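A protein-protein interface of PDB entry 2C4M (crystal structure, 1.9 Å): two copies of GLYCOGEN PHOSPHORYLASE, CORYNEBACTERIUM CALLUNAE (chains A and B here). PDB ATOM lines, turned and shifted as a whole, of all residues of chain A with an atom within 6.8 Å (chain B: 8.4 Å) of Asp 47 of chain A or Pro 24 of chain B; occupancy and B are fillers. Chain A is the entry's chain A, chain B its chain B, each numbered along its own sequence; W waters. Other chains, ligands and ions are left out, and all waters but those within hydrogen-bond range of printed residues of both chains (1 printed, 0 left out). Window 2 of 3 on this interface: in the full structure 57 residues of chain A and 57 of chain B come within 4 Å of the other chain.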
ATOM      1  N   GLN A  42     -32.854 -20.311  17.501  1.00  0.00           N
ATOM      2  CA  GLN A  42     -31.544 -20.299  18.141  1.00  0.00           C
ATOM      3  C   GLN A  42     -31.308 -18.990  18.870  1.00  0.00           C
ATOM      4  O   GLN A  42     -30.725 -18.958  19.950  1.00  0.00           O
ATOM      5  CB  GLN A  42     -30.432 -20.483  17.101  1.00  0.00           C
ATOM      6  CG  GLN A  42     -30.236 -21.908  16.625  1.00  0.00           C
ATOM      7  CD  GLN A  42     -29.765 -22.818  17.741  1.00  0.00           C
ATOM      8  OE1 GLN A  42     -30.269 -22.750  18.862  1.00  0.00           O
ATOM      9  NE2 GLN A  42     -28.800 -23.686  17.440  1.00  0.00           N
ATOM     10  N   GLU A  43     -31.757 -17.904  18.264  1.00  0.00           N
ATOM     11  CA  GLU A  43     -31.653 -16.573  18.830  1.00  0.00           C
ATOM     12  C   GLU A  43     -32.369 -16.511  20.171  1.00  0.00           C
ATOM     13  O   GLU A  43     -31.868 -15.969  21.147  1.00  0.00           O
ATOM     14  CB  GLU A  43     -32.291 -15.587  17.851  1.00  0.00           C
ATOM     15  CG  GLU A  43     -32.011 -14.130  18.226  1.00  0.00           C
ATOM     16  CD  GLU A  43     -33.086 -13.641  19.169  1.00  0.00           C
ATOM     17  OE1 GLU A  43     -34.205 -14.125  19.086  1.00  0.00           O
ATOM     18  OE2 GLU A  43     -32.790 -12.769  19.986  1.00  0.00           O
ATOM     19  N   ARG A  44     -33.582 -17.058  20.182  1.00  0.00           N
ATOM     20  CA  ARG A  44     -34.436 -16.990  21.370  1.00  0.00           C
ATOM     21  C   ARG A  44     -33.944 -17.824  22.550  1.00  0.00           C
ATOM     22  O   ARG A  44     -34.181 -17.453  23.702  1.00  0.00           O
ATOM     23  CB  ARG A  44     -35.835 -17.470  20.954  1.00  0.00           C
ATOM     24  N   ILE A  45     -33.256 -18.935  22.284  1.00  0.00           N
ATOM     25  CA  ILE A  45     -32.786 -19.774  23.384  1.00  0.00           C
ATOM     26  C   ILE A  45     -31.341 -19.526  23.789  1.00  0.00           C
ATOM     27  O   ILE A  45     -30.893 -20.015  24.822  1.00  0.00           O
ATOM     28  CB  ILE A  45     -32.962 -21.267  23.057  1.00  0.00           C
ATOM     29  CG1 ILE A  45     -31.844 -21.745  22.132  1.00  0.00           C
ATOM     30  CG2 ILE A  45     -34.312 -21.481  22.403  1.00  0.00           C
ATOM     31  CD1 ILE A  45     -32.013 -23.183  21.668  1.00  0.00           C
ATOM     32  N   ALA A  46     -30.619 -18.755  22.982  1.00  0.00           N
ATOM     33  CA  ALA A  46     -29.212 -18.450  23.255  1.00  0.00           C
ATOM     34  C   ALA A  46     -28.948 -18.072  24.709  1.00  0.00           C
ATOM     35  O   ALA A  46     -28.021 -18.591  25.334  1.00  0.00           O
ATOM     36  CB  ALA A  46     -28.735 -17.321  22.340  1.00  0.00           C
ATOM     37  N   ASP A  47     -29.751 -17.153  25.242  1.00  0.00           N
ATOM     38  CA  ASP A  47     -29.577 -16.718  26.622  1.00  0.00           C
ATOM     39  C   ASP A  47     -29.739 -17.850  27.625  1.00  0.00           C
ATOM     40  O   ASP A  47     -28.876 -18.044  28.482  1.00  0.00           O
ATOM     41  CB  ASP A  47     -30.553 -15.582  26.948  1.00  0.00           C
ATOM     42  CG  ASP A  47     -29.980 -14.207  26.615  1.00  0.00           C
ATOM     43  OD1 ASP A  47     -29.184 -13.677  27.430  1.00  0.00           O
ATOM     44  OD2 ASP A  47     -30.313 -13.663  25.538  1.00  0.00           O
ATOM     45  N   ASP A  48     -30.841 -18.586  27.525  1.00  0.00           N
ATOM     46  CA  ASP A  48     -31.147 -19.735  28.366  1.00  0.00           C
ATOM     47  C   ASP A  48     -30.062 -20.807  28.262  1.00  0.00           C
ATOM     48  O   ASP A  48     -29.717 -21.475  29.228  1.00  0.00           O
ATOM     49  CB  ASP A  48     -32.493 -20.308  27.920  1.00  0.00           C
ATOM     50  CG  ASP A  48     -33.617 -19.530  28.589  1.00  0.00           C
ATOM     51  OD1 ASP A  48     -33.332 -18.837  29.566  1.00  0.00           O
ATOM     52  OD2 ASP A  48     -34.753 -19.621  28.131  1.00  0.00           O
ATOM     53  N   TRP A  49     -29.600 -20.987  27.032  1.00  0.00           N
ATOM     54  CA  TRP A  49     -28.601 -22.017  26.766  1.00  0.00           C
ATOM     55  C   TRP A  49     -27.340 -21.679  27.553  1.00  0.00           C
ATOM     56  O   TRP A  49     -26.757 -22.534  28.213  1.00  0.00           O
ATOM     57  CB  TRP A  49     -28.290 -22.072  25.267  1.00  0.00           C
ATOM     58  CG  TRP A  49     -27.616 -23.352  24.817  1.00  0.00           C
ATOM     59  CD1 TRP A  49     -27.210 -24.396  25.605  1.00  0.00           C
ATOM     60  CD2 TRP A  49     -27.251 -23.697  23.475  1.00  0.00           C
ATOM     61  NE1 TRP A  49     -26.611 -25.371  24.831  1.00  0.00           N
ATOM     62  CE2 TRP A  49     -26.624 -24.966  23.521  1.00  0.00           C
ATOM     63  CE3 TRP A  49     -27.393 -23.057  22.237  1.00  0.00           C
ATOM     64  CZ2 TRP A  49     -26.137 -25.607  22.376  1.00  0.00           C
ATOM     65  CZ3 TRP A  49     -26.908 -23.693  21.094  1.00  0.00           C
ATOM     66  CH2 TRP A  49     -26.288 -24.956  21.174  1.00  0.00           C
ATOM     67  N   GLU A  50     -26.935 -20.410  27.507  1.00  0.00           N
ATOM     68  CA  GLU A  50     -25.760 -19.978  28.253  1.00  0.00           C
ATOM     69  C   GLU A  50     -25.953 -20.116  29.770  1.00  0.00           C
ATOM     70  O   GLU A  50     -25.053 -20.533  30.487  1.00  0.00           O
ATOM     71  CB  GLU A  50     -25.409 -18.533  27.865  1.00  0.00           C
ATOM     72  CG  GLU A  50     -24.216 -17.966  28.645  1.00  0.00           C
ATOM     73  CD  GLU A  50     -22.942 -18.730  28.320  1.00  0.00           C
ATOM     74  OE1 GLU A  50     -22.783 -19.145  27.177  1.00  0.00           O
ATOM     75  OE2 GLU A  50     -22.083 -18.822  29.195  1.00  0.00           O
ATOM     76  N   ARG A  51     -27.181 -19.869  30.239  1.00  0.00           N
ATOM     77  CA  ARG A  51     -27.399 -19.881  31.679  1.00  0.00           C
ATOM     78  C   ARG A  51     -27.270 -21.306  32.194  1.00  0.00           C
ATOM     79  O   ARG A  51     -26.632 -21.590  33.202  1.00  0.00           O
ATOM     80  CB  ARG A  51     -28.783 -19.293  31.990  1.00  0.00           C
ATOM     81  CG  ARG A  51     -28.861 -17.803  31.671  1.00  0.00           C
ATOM     82  CD  ARG A  51     -30.132 -17.164  32.242  1.00  0.00           C
ATOM     83  NE  ARG A  51     -30.332 -15.825  31.682  1.00  0.00           N
ATOM     84  CZ  ARG A  51     -31.366 -15.659  30.836  1.00  0.00           C
ATOM     85  NH1 ARG A  51     -32.160 -16.675  30.549  1.00  0.00           N
ATOM     86  NH2 ARG A  51     -31.587 -14.459  30.292  1.00  0.00           N
ATOM     87  N   THR A  52     -27.807 -22.197  31.328  1.00  0.00           N
ATOM     88  CA  THR A  52     -27.687 -23.618  31.572  1.00  0.00           C
ATOM     89  C   THR A  52     -26.244 -24.076  31.621  1.00  0.00           C
ATOM     90  O   THR A  52     -25.838 -24.831  32.496  1.00  0.00           O
ATOM     91  CB  THR A  52     -28.460 -24.427  30.529  1.00  0.00           C
ATOM     92  OG1 THR A  52     -29.793 -23.913  30.391  1.00  0.00           O
ATOM     93  CG2 THR A  52     -28.558 -25.887  30.979  1.00  0.00           C
ATOM     94  N   ARG A  53     -25.429 -23.538  30.669  1.00  0.00           N
ATOM     95  CA  ARG A  53     -24.017 -23.915  30.662  1.00  0.00           C
ATOM     96  C   ARG A  53     -23.349 -23.537  31.977  1.00  0.00           C
ATOM     97  O   ARG A  53     -22.543 -24.288  32.510  1.00  0.00           O
ATOM     98  CB  ARG A  53     -23.280 -23.156  29.575  1.00  0.00           C
ATOM     99  CG  ARG A  53     -23.710 -23.516  28.150  1.00  0.00           C
ATOM    100  CD  ARG A  53     -22.692 -22.972  27.138  1.00  0.00           C
ATOM    101  NE  ARG A  53     -23.099 -23.304  25.774  1.00  0.00           N
ATOM    102  CZ  ARG A  53     -23.761 -22.365  25.034  1.00  0.00           C
ATOM    103  NH1 ARG A  53     -24.019 -21.137  25.512  1.00  0.00           N
ATOM    104  NH2 ARG A  53     -24.179 -22.700  23.823  1.00  0.00           N
ATOM    105  N   GLU A  54     -23.661 -22.351  32.491  1.00  0.00           N
ATOM    106  CA  GLU A  54     -23.049 -21.896  33.726  1.00  0.00           C
ATOM    107  C   GLU A  54     -23.548 -22.702  34.914  1.00  0.00           C
ATOM    108  O   GLU A  54     -22.780 -23.042  35.809  1.00  0.00           O
ATOM    109  CB  GLU A  54     -23.340 -20.407  33.939  1.00  0.00           C
ATOM    110  CG  GLU A  54     -22.796 -19.551  32.812  1.00  0.00           C
ATOM    111  CD  GLU A  54     -23.037 -18.068  33.005  1.00  0.00           C
ATOM    112  OE1 GLU A  54     -24.213 -17.642  33.014  1.00  0.00           O
ATOM    113  OE2 GLU A  54     -22.043 -17.328  33.143  1.00  0.00           O
ATOM    114  N   HIS A 202     -36.662 -23.971  31.193  1.00  0.00           N
ATOM    115  CA  HIS A 202     -35.861 -23.025  30.423  1.00  0.00           C
ATOM    116  C   HIS A 202     -34.475 -23.603  30.151  1.00  0.00           C
ATOM    117  O   HIS A 202     -33.708 -23.056  29.355  1.00  0.00           O
ATOM    118  CB  HIS A 202     -35.724 -21.700  31.171  1.00  0.00           C
ATOM    119  CG  HIS A 202     -36.971 -20.879  31.155  1.00  0.00           C
ATOM    120  ND1 HIS A 202     -37.531 -20.409  29.987  1.00  0.00           N
ATOM    121  CD2 HIS A 202     -37.778 -20.459  32.157  1.00  0.00           C
ATOM    122  CE1 HIS A 202     -38.631 -19.733  30.271  1.00  0.00           C
ATOM    123  NE2 HIS A 202     -38.802 -19.749  31.580  1.00  0.00           N
ATOM    124  N   ALA A 793     -31.470 -23.575  35.293  1.00  0.00           N
ATOM    125  CA  ALA A 793     -30.630 -22.477  34.831  1.00  0.00           C
ATOM    126  C   ALA A 793     -31.092 -21.161  35.443  1.00  0.00           C
ATOM    127  O   ALA A 793     -32.241 -21.002  35.808  1.00  0.00           O
ATOM    128  CB  ALA A 793     -30.748 -22.399  33.305  1.00  0.00           C
ATOM    129  N   GLY B  14     -27.183  -7.936  17.555  1.00  0.00           N
ATOM    130  CA  GLY B  14     -27.201  -8.919  18.623  1.00  0.00           C
ATOM    131  C   GLY B  14     -28.089 -10.109  18.271  1.00  0.00           C
ATOM    132  O   GLY B  14     -27.761 -11.245  18.588  1.00  0.00           O
ATOM    133  N   SER B  15     -29.211  -9.854  17.610  1.00  0.00           N
ATOM    134  CA  SER B  15     -30.113 -10.937  17.219  1.00  0.00           C
ATOM    135  C   SER B  15     -29.405 -11.967  16.336  1.00  0.00           C
ATOM    136  O   SER B  15     -29.427 -13.169  16.584  1.00  0.00           O
ATOM    137  CB  SER B  15     -31.310 -10.338  16.472  1.00  0.00           C
ATOM    138  OG  SER B  15     -32.335 -11.322  16.335  1.00  0.00           O
ATOM    139  N   VAL B  17     -26.134 -12.280  15.884  1.00  0.00           N
ATOM    140  CA  VAL B  17     -24.982 -12.891  16.531  1.00  0.00           C
ATOM    141  C   VAL B  17     -25.417 -14.040  17.435  1.00  0.00           C
ATOM    142  O   VAL B  17     -24.824 -15.110  17.430  1.00  0.00           O
ATOM    143  CB  VAL B  17     -24.222 -11.831  17.333  1.00  0.00           C
ATOM    144  CG1 VAL B  17     -23.103 -12.491  18.137  1.00  0.00           C
ATOM    145  CG2 VAL B  17     -23.620 -10.801  16.396  1.00  0.00           C
ATOM    146  N   ARG B  18     -26.488 -13.832  18.202  1.00  0.00           N
ATOM    147  CA  ARG B  18     -26.995 -14.870  19.102  1.00  0.00           C
ATOM    148  C   ARG B  18     -27.382 -16.114  18.314  1.00  0.00           C
ATOM    149  O   ARG B  18     -27.118 -17.231  18.748  1.00  0.00           O
ATOM    150  CB  ARG B  18     -28.225 -14.373  19.891  1.00  0.00           C
ATOM    151  CG  ARG B  18     -27.916 -13.426  21.048  1.00  0.00           C
ATOM    152  CD  ARG B  18     -29.140 -13.225  21.960  1.00  0.00           C
ATOM    153  NE  ARG B  18     -30.257 -12.574  21.274  1.00  0.00           N
ATOM    154  CZ  ARG B  18     -30.308 -11.274  20.974  1.00  0.00           C
ATOM    155  NH1 ARG B  18     -29.307 -10.464  21.299  1.00  0.00           N
ATOM    156  NH2 ARG B  18     -31.363 -10.780  20.342  1.00  0.00           N
ATOM    157  N   ALA B  19     -27.999 -15.920  17.153  1.00  0.00           N
ATOM    158  CA  ALA B  19     -28.421 -17.050  16.333  1.00  0.00           C
ATOM    159  C   ALA B  19     -27.217 -17.835  15.828  1.00  0.00           C
ATOM    160  O   ALA B  19     -27.259 -19.064  15.729  1.00  0.00           O
ATOM    161  CB  ALA B  19     -29.264 -16.564  15.154  1.00  0.00           C
ATOM    162  N   ALA B  21     -24.090 -17.766  17.310  1.00  0.00           N
ATOM    163  CA  ALA B  21     -23.279 -18.233  18.425  1.00  0.00           C
ATOM    164  C   ALA B  21     -23.915 -19.117  19.491  1.00  0.00           C
ATOM    165  O   ALA B  21     -23.192 -19.739  20.268  1.00  0.00           O
ATOM    166  CB  ALA B  21     -22.614 -17.026  19.098  1.00  0.00           C
ATOM    167  N   GLY B  22     -25.242 -19.174  19.548  1.00  0.00           N
ATOM    168  CA  GLY B  22     -25.882 -19.985  20.569  1.00  0.00           C
ATOM    169  C   GLY B  22     -25.453 -19.494  21.943  1.00  0.00           C
ATOM    170  O   GLY B  22     -25.294 -20.273  22.885  1.00  0.00           O
ATOM    171  N   THR B  23     -25.265 -18.183  22.057  1.00  0.00           N
ATOM    172  CA  THR B  23     -24.836 -17.570  23.311  1.00  0.00           C
ATOM    173  C   THR B  23     -25.087 -16.059  23.194  1.00  0.00           C
ATOM    174  O   THR B  23     -25.151 -15.525  22.087  1.00  0.00           O
ATOM    175  CB  THR B  23     -23.329 -17.850  23.549  1.00  0.00           C
ATOM    176  OG1 THR B  23     -23.025 -17.716  24.943  1.00  0.00           O
ATOM    177  CG2 THR B  23     -22.458 -16.883  22.734  1.00  0.00           C
ATOM    178  N   PRO B  24     -25.264 -15.356  24.326  1.00  0.00           N
ATOM    179  CA  PRO B  24     -25.501 -13.908  24.208  1.00  0.00           C
ATOM    180  C   PRO B  24     -24.402 -13.236  23.392  1.00  0.00           C
ATOM    181  O   PRO B  24     -23.235 -13.594  23.495  1.00  0.00           O
ATOM    182  CB  PRO B  24     -25.643 -13.449  25.663  1.00  0.00           C
ATOM    183  CG  PRO B  24     -25.067 -14.544  26.519  1.00  0.00           C
ATOM    184  CD  PRO B  24     -25.324 -15.790  25.731  1.00  0.00           C
ATOM    185  N   ALA B  25     -24.783 -12.255  22.583  1.00  0.00           N
ATOM    186  CA  ALA B  25     -23.847 -11.557  21.711  1.00  0.00           C
ATOM    187  C   ALA B  25     -22.542 -11.098  22.343  1.00  0.00           C
ATOM    188  O   ALA B  25     -21.485 -11.185  21.724  1.00  0.00           O
ATOM    189  CB  ALA B  25     -24.550 -10.379  21.071  1.00  0.00           C
ATOM    190  N   ASP B  26     -22.611 -10.607  23.575  1.00  0.00           N
ATOM    191  CA  ASP B  26     -21.428 -10.109  24.278  1.00  0.00           C
ATOM    192  C   ASP B  26     -20.454 -11.214  24.667  1.00  0.00           C
ATOM    193  O   ASP B  26     -19.291 -10.966  25.006  1.00  0.00           O
ATOM    194  CB  ASP B  26     -21.869  -9.331  25.518  1.00  0.00           C
ATOM    195  CG  ASP B  26     -23.064  -9.958  26.190  1.00  0.00           C
ATOM    196  OD1 ASP B  26     -24.207  -9.632  25.793  1.00  0.00           O
ATOM    197  OD2 ASP B  26     -22.851 -10.788  27.098  1.00  0.00           O
ATOM    198  N   LEU B  27     -20.930 -12.449  24.627  1.00  0.00           N
ATOM    199  CA  LEU B  27     -20.069 -13.569  24.972  1.00  0.00           C
ATOM    200  C   LEU B  27     -19.593 -14.317  23.720  1.00  0.00           C
ATOM    201  O   LEU B  27     -18.758 -15.207  23.808  1.00  0.00           O
ATOM    202  CB  LEU B  27     -20.804 -14.521  25.925  1.00  0.00           C
ATOM    203  CG  LEU B  27     -21.072 -13.928  27.319  1.00  0.00           C
ATOM    204  CD1 LEU B  27     -21.873 -14.918  28.173  1.00  0.00           C
ATOM    205  CD2 LEU B  27     -19.741 -13.598  27.984  1.00  0.00           C
ATOM    206  N   ALA B  28     -20.138 -13.956  22.566  1.00  0.00           N
ATOM    207  CA  ALA B  28     -19.762 -14.597  21.308  1.00  0.00           C
ATOM    208  C   ALA B  28     -18.286 -14.376  20.970  1.00  0.00           C
ATOM    209  O   ALA B  28     -17.702 -13.346  21.319  1.00  0.00           O
ATOM    210  CB  ALA B  28     -20.640 -14.055  20.170  1.00  0.00           C
ATOM    211  N   THR B  29     -17.677 -15.347  20.300  1.00  0.00           N
ATOM    212  CA  THR B  29     -16.284 -15.208  19.889  1.00  0.00           C
ATOM    213  C   THR B  29     -16.272 -14.186  18.738  1.00  0.00           C
ATOM    214  O   THR B  29     -17.315 -13.878  18.167  1.00  0.00           O
ATOM    215  CB  THR B  29     -15.726 -16.531  19.327  1.00  0.00           C
ATOM    216  OG1 THR B  29     -16.476 -16.889  18.164  1.00  0.00           O
ATOM    217  CG2 THR B  29     -15.812 -17.654  20.355  1.00  0.00           C
ATOM    218  N   LYS B  32     -17.833 -15.674  15.539  1.00  0.00           N
ATOM    219  CA  LYS B  32     -19.289 -15.701  15.516  1.00  0.00           C
ATOM    220  C   LYS B  32     -19.864 -14.298  15.404  1.00  0.00           C
ATOM    221  O   LYS B  32     -20.890 -14.098  14.760  1.00  0.00           O
ATOM    222  CB  LYS B  32     -19.830 -16.399  16.768  1.00  0.00           C
ATOM    223  CG  LYS B  32     -19.535 -17.898  16.794  1.00  0.00           C
ATOM    224  CD  LYS B  32     -20.209 -18.616  15.649  1.00  0.00           C
ATOM    225  CE  LYS B  32     -19.968 -20.127  15.714  1.00  0.00           C
ATOM    226  NZ  LYS B  32     -18.548 -20.489  15.416  1.00  0.00           N
ATOM    227  N   PHE B  33     -19.211 -13.323  16.027  1.00  0.00           N
ATOM    228  CA  PHE B  33     -19.710 -11.961  15.946  1.00  0.00           C
ATOM    229  C   PHE B  33     -19.620 -11.477  14.497  1.00  0.00           C
ATOM    230  O   PHE B  33     -20.572 -10.899  13.967  1.00  0.00           O
ATOM    231  CB  PHE B  33     -18.925 -11.032  16.871  1.00  0.00           C
ATOM    232  CG  PHE B  33     -19.614  -9.728  17.120  1.00  0.00           C
ATOM    233  CD1 PHE B  33     -19.601  -8.720  16.159  1.00  0.00           C
ATOM    234  CD2 PHE B  33     -20.342  -9.529  18.287  1.00  0.00           C
ATOM    235  CE1 PHE B  33     -20.309  -7.536  16.358  1.00  0.00           C
ATOM    236  CE2 PHE B  33     -21.051  -8.347  18.495  1.00  0.00           C
ATOM    237  CZ  PHE B  33     -21.033  -7.350  17.526  1.00  0.00           C
ATOM    238  N   LEU B  95     -22.053  -4.024  22.153  1.00  0.00           N
ATOM    239  CA  LEU B  95     -22.180  -5.458  22.399  1.00  0.00           C
ATOM    240  C   LEU B  95     -20.879  -6.133  22.827  1.00  0.00           C
ATOM    241  O   LEU B  95     -20.687  -7.328  22.594  1.00  0.00           O
ATOM    242  CB  LEU B  95     -22.741  -6.147  21.152  1.00  0.00           C
ATOM    243  CG  LEU B  95     -24.132  -5.684  20.711  1.00  0.00           C
ATOM    244  CD1 LEU B  95     -24.418  -6.157  19.302  1.00  0.00           C
ATOM    245  CD2 LEU B  95     -25.185  -6.203  21.680  1.00  0.00           C
ATOM    246  N   HIS B  97     -17.651  -5.919  21.741  1.00  0.00           N
ATOM    247  CA  HIS B  97     -16.542  -6.234  20.842  1.00  0.00           C
ATOM    248  C   HIS B  97     -15.975  -4.983  20.174  1.00  0.00           C
ATOM    249  O   HIS B  97     -16.519  -3.888  20.330  1.00  0.00           O
ATOM    250  CB  HIS B  97     -17.001  -7.230  19.770  1.00  0.00           C
ATOM    251  CG  HIS B  97     -17.399  -8.571  20.314  1.00  0.00           C
ATOM    252  ND1 HIS B  97     -18.524  -8.758  21.092  1.00  0.00           N
ATOM    253  CD2 HIS B  97     -16.815  -9.789  20.200  1.00  0.00           C
ATOM    254  CE1 HIS B  97     -18.614 -10.032  21.434  1.00  0.00           C
ATOM    255  NE2 HIS B  97     -17.590 -10.679  20.905  1.00  0.00           N
HETATM  256  O   HOH W   1     -20.228 -18.376  25.746  1.00  0.00           O
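No position is printed for both chains. Of the 16 pairs that touch across the chains among the printed residues, none has its exchanged pair printed and touching as well.
The side-chain carboxylate of Glu 43 of chain A lies within salt-bridge range of the guanidinium group of Arg 18 of chain B, 2.5 Å away. The side-chain hydroxyl (OG1) of Thr 23 of chain B sits at hydrogen-bond distance from the side-chain carboxylate (OE1) of Glu 50 of chain A (2.7 Å). The guanidinium group (NH2) of Arg 53 of chain A sits at hydrogen-bond distance from the backbone carbonyl oxygen (O) of Gly 22 of chain B, 2.8 Å away.
Asp 47 of chain A touches just these residues of chain B: Arg 18 and Pro 24. Pro 24 of chain B touches just these residues of chain A: Ala 46 (3.9 Å), Asp 47 (3.96 Å) and Glu 50 (3.5 Å). Printed residues of chain B within 4 Å of Glu 43 of chain A: Ser 15, Arg 18 and Ala 19. Of the printed residues of chain A, Thr 23 of chain B touches Ala 46 (3.6 Å), Glu 50 (2.7 Å) and Arg 53 (3.6 Å). Printed residues of chain B within 4 Å of Arg 53 of chain A: Gly 22 and Thr 23. The nearest residue of chain B that does not touch Asp 47 of chain A is Thr 23 of chain B (5.2 Å). The nearest printed residue of chain B that does not touch Gln 42 of chain A is Arg 18 of chain B (4.2 Å).
The guanidinium group of Arg 51 of chain A lies within salt-bridge range of the side-chain carboxylate of Asp 47 of chain A, at 3.8 Å. OE1 of Glu 50 of chain A is in salt-bridge range of NH1 of Arg 53 of chain A (2.9 Å). The guanidinium group (NH1) of Arg 18 of chain B sits at hydrogen-bond distance from the backbone carbonyl oxygen (O) of Gly 14 of chain B, at 3.2 Å.
Among the printed residues, pairs that only touch across the chains: Glu 43 of chain A with Ser 15 of chain B, Glu 50 of chain A with Pro 24 of chain B, Trp 49 of chain A with Gly 22 of chain B, Ala 46 of chain A with Thr 23 of chain B, Arg 53 of chain A with Thr 23 of chain B, Gln 42 of chain A with Ala 19 of chain B, Asp 47 of chain A with Arg 18 of chain B, Ala 46 of chain A with Arg 18 of chain B, Glu 50 of chain A with Leu 27 of chain B, Ala 46 of chain A with Pro 24 of chain B, Glu 43 of chain A with Ala 19 of chain B, Ala 46 of chain A with Gly 22 of chain B and Asp 47 of chain A with Pro 24 of chain B.
Of the 15 printed residues of chain A, 7 touch a printed residue of chain B. Printed residues of chain A that touch a printed residue of chain B: Gln 42, Glu 43, Ala 46, Asp 47, Trp 49, Glu 50 and Arg 53. Hydrophobic or aromatic side chains of chain A that line the printed part of chain B: Ala 46 and Trp 49. Along chain A the printed residues that touch a printed residue of chain B span positions 42 to 53. Among the printed residues, 16 pairs touch across the chains. Among the printed residues, Asp or Glu carboxylates within 4 Å of a Lys or Arg side-chain nitrogen of the other chain: Glu 43 of chain A with Arg 18 of chain B (2.5 Å).
Water W1 bridges the side-chain hydroxyl (OG1) of Thr 23 of chain B (3.0 Å) and the side-chain carboxylate (OE1) of Glu 50 of chain A (3.0 Å).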
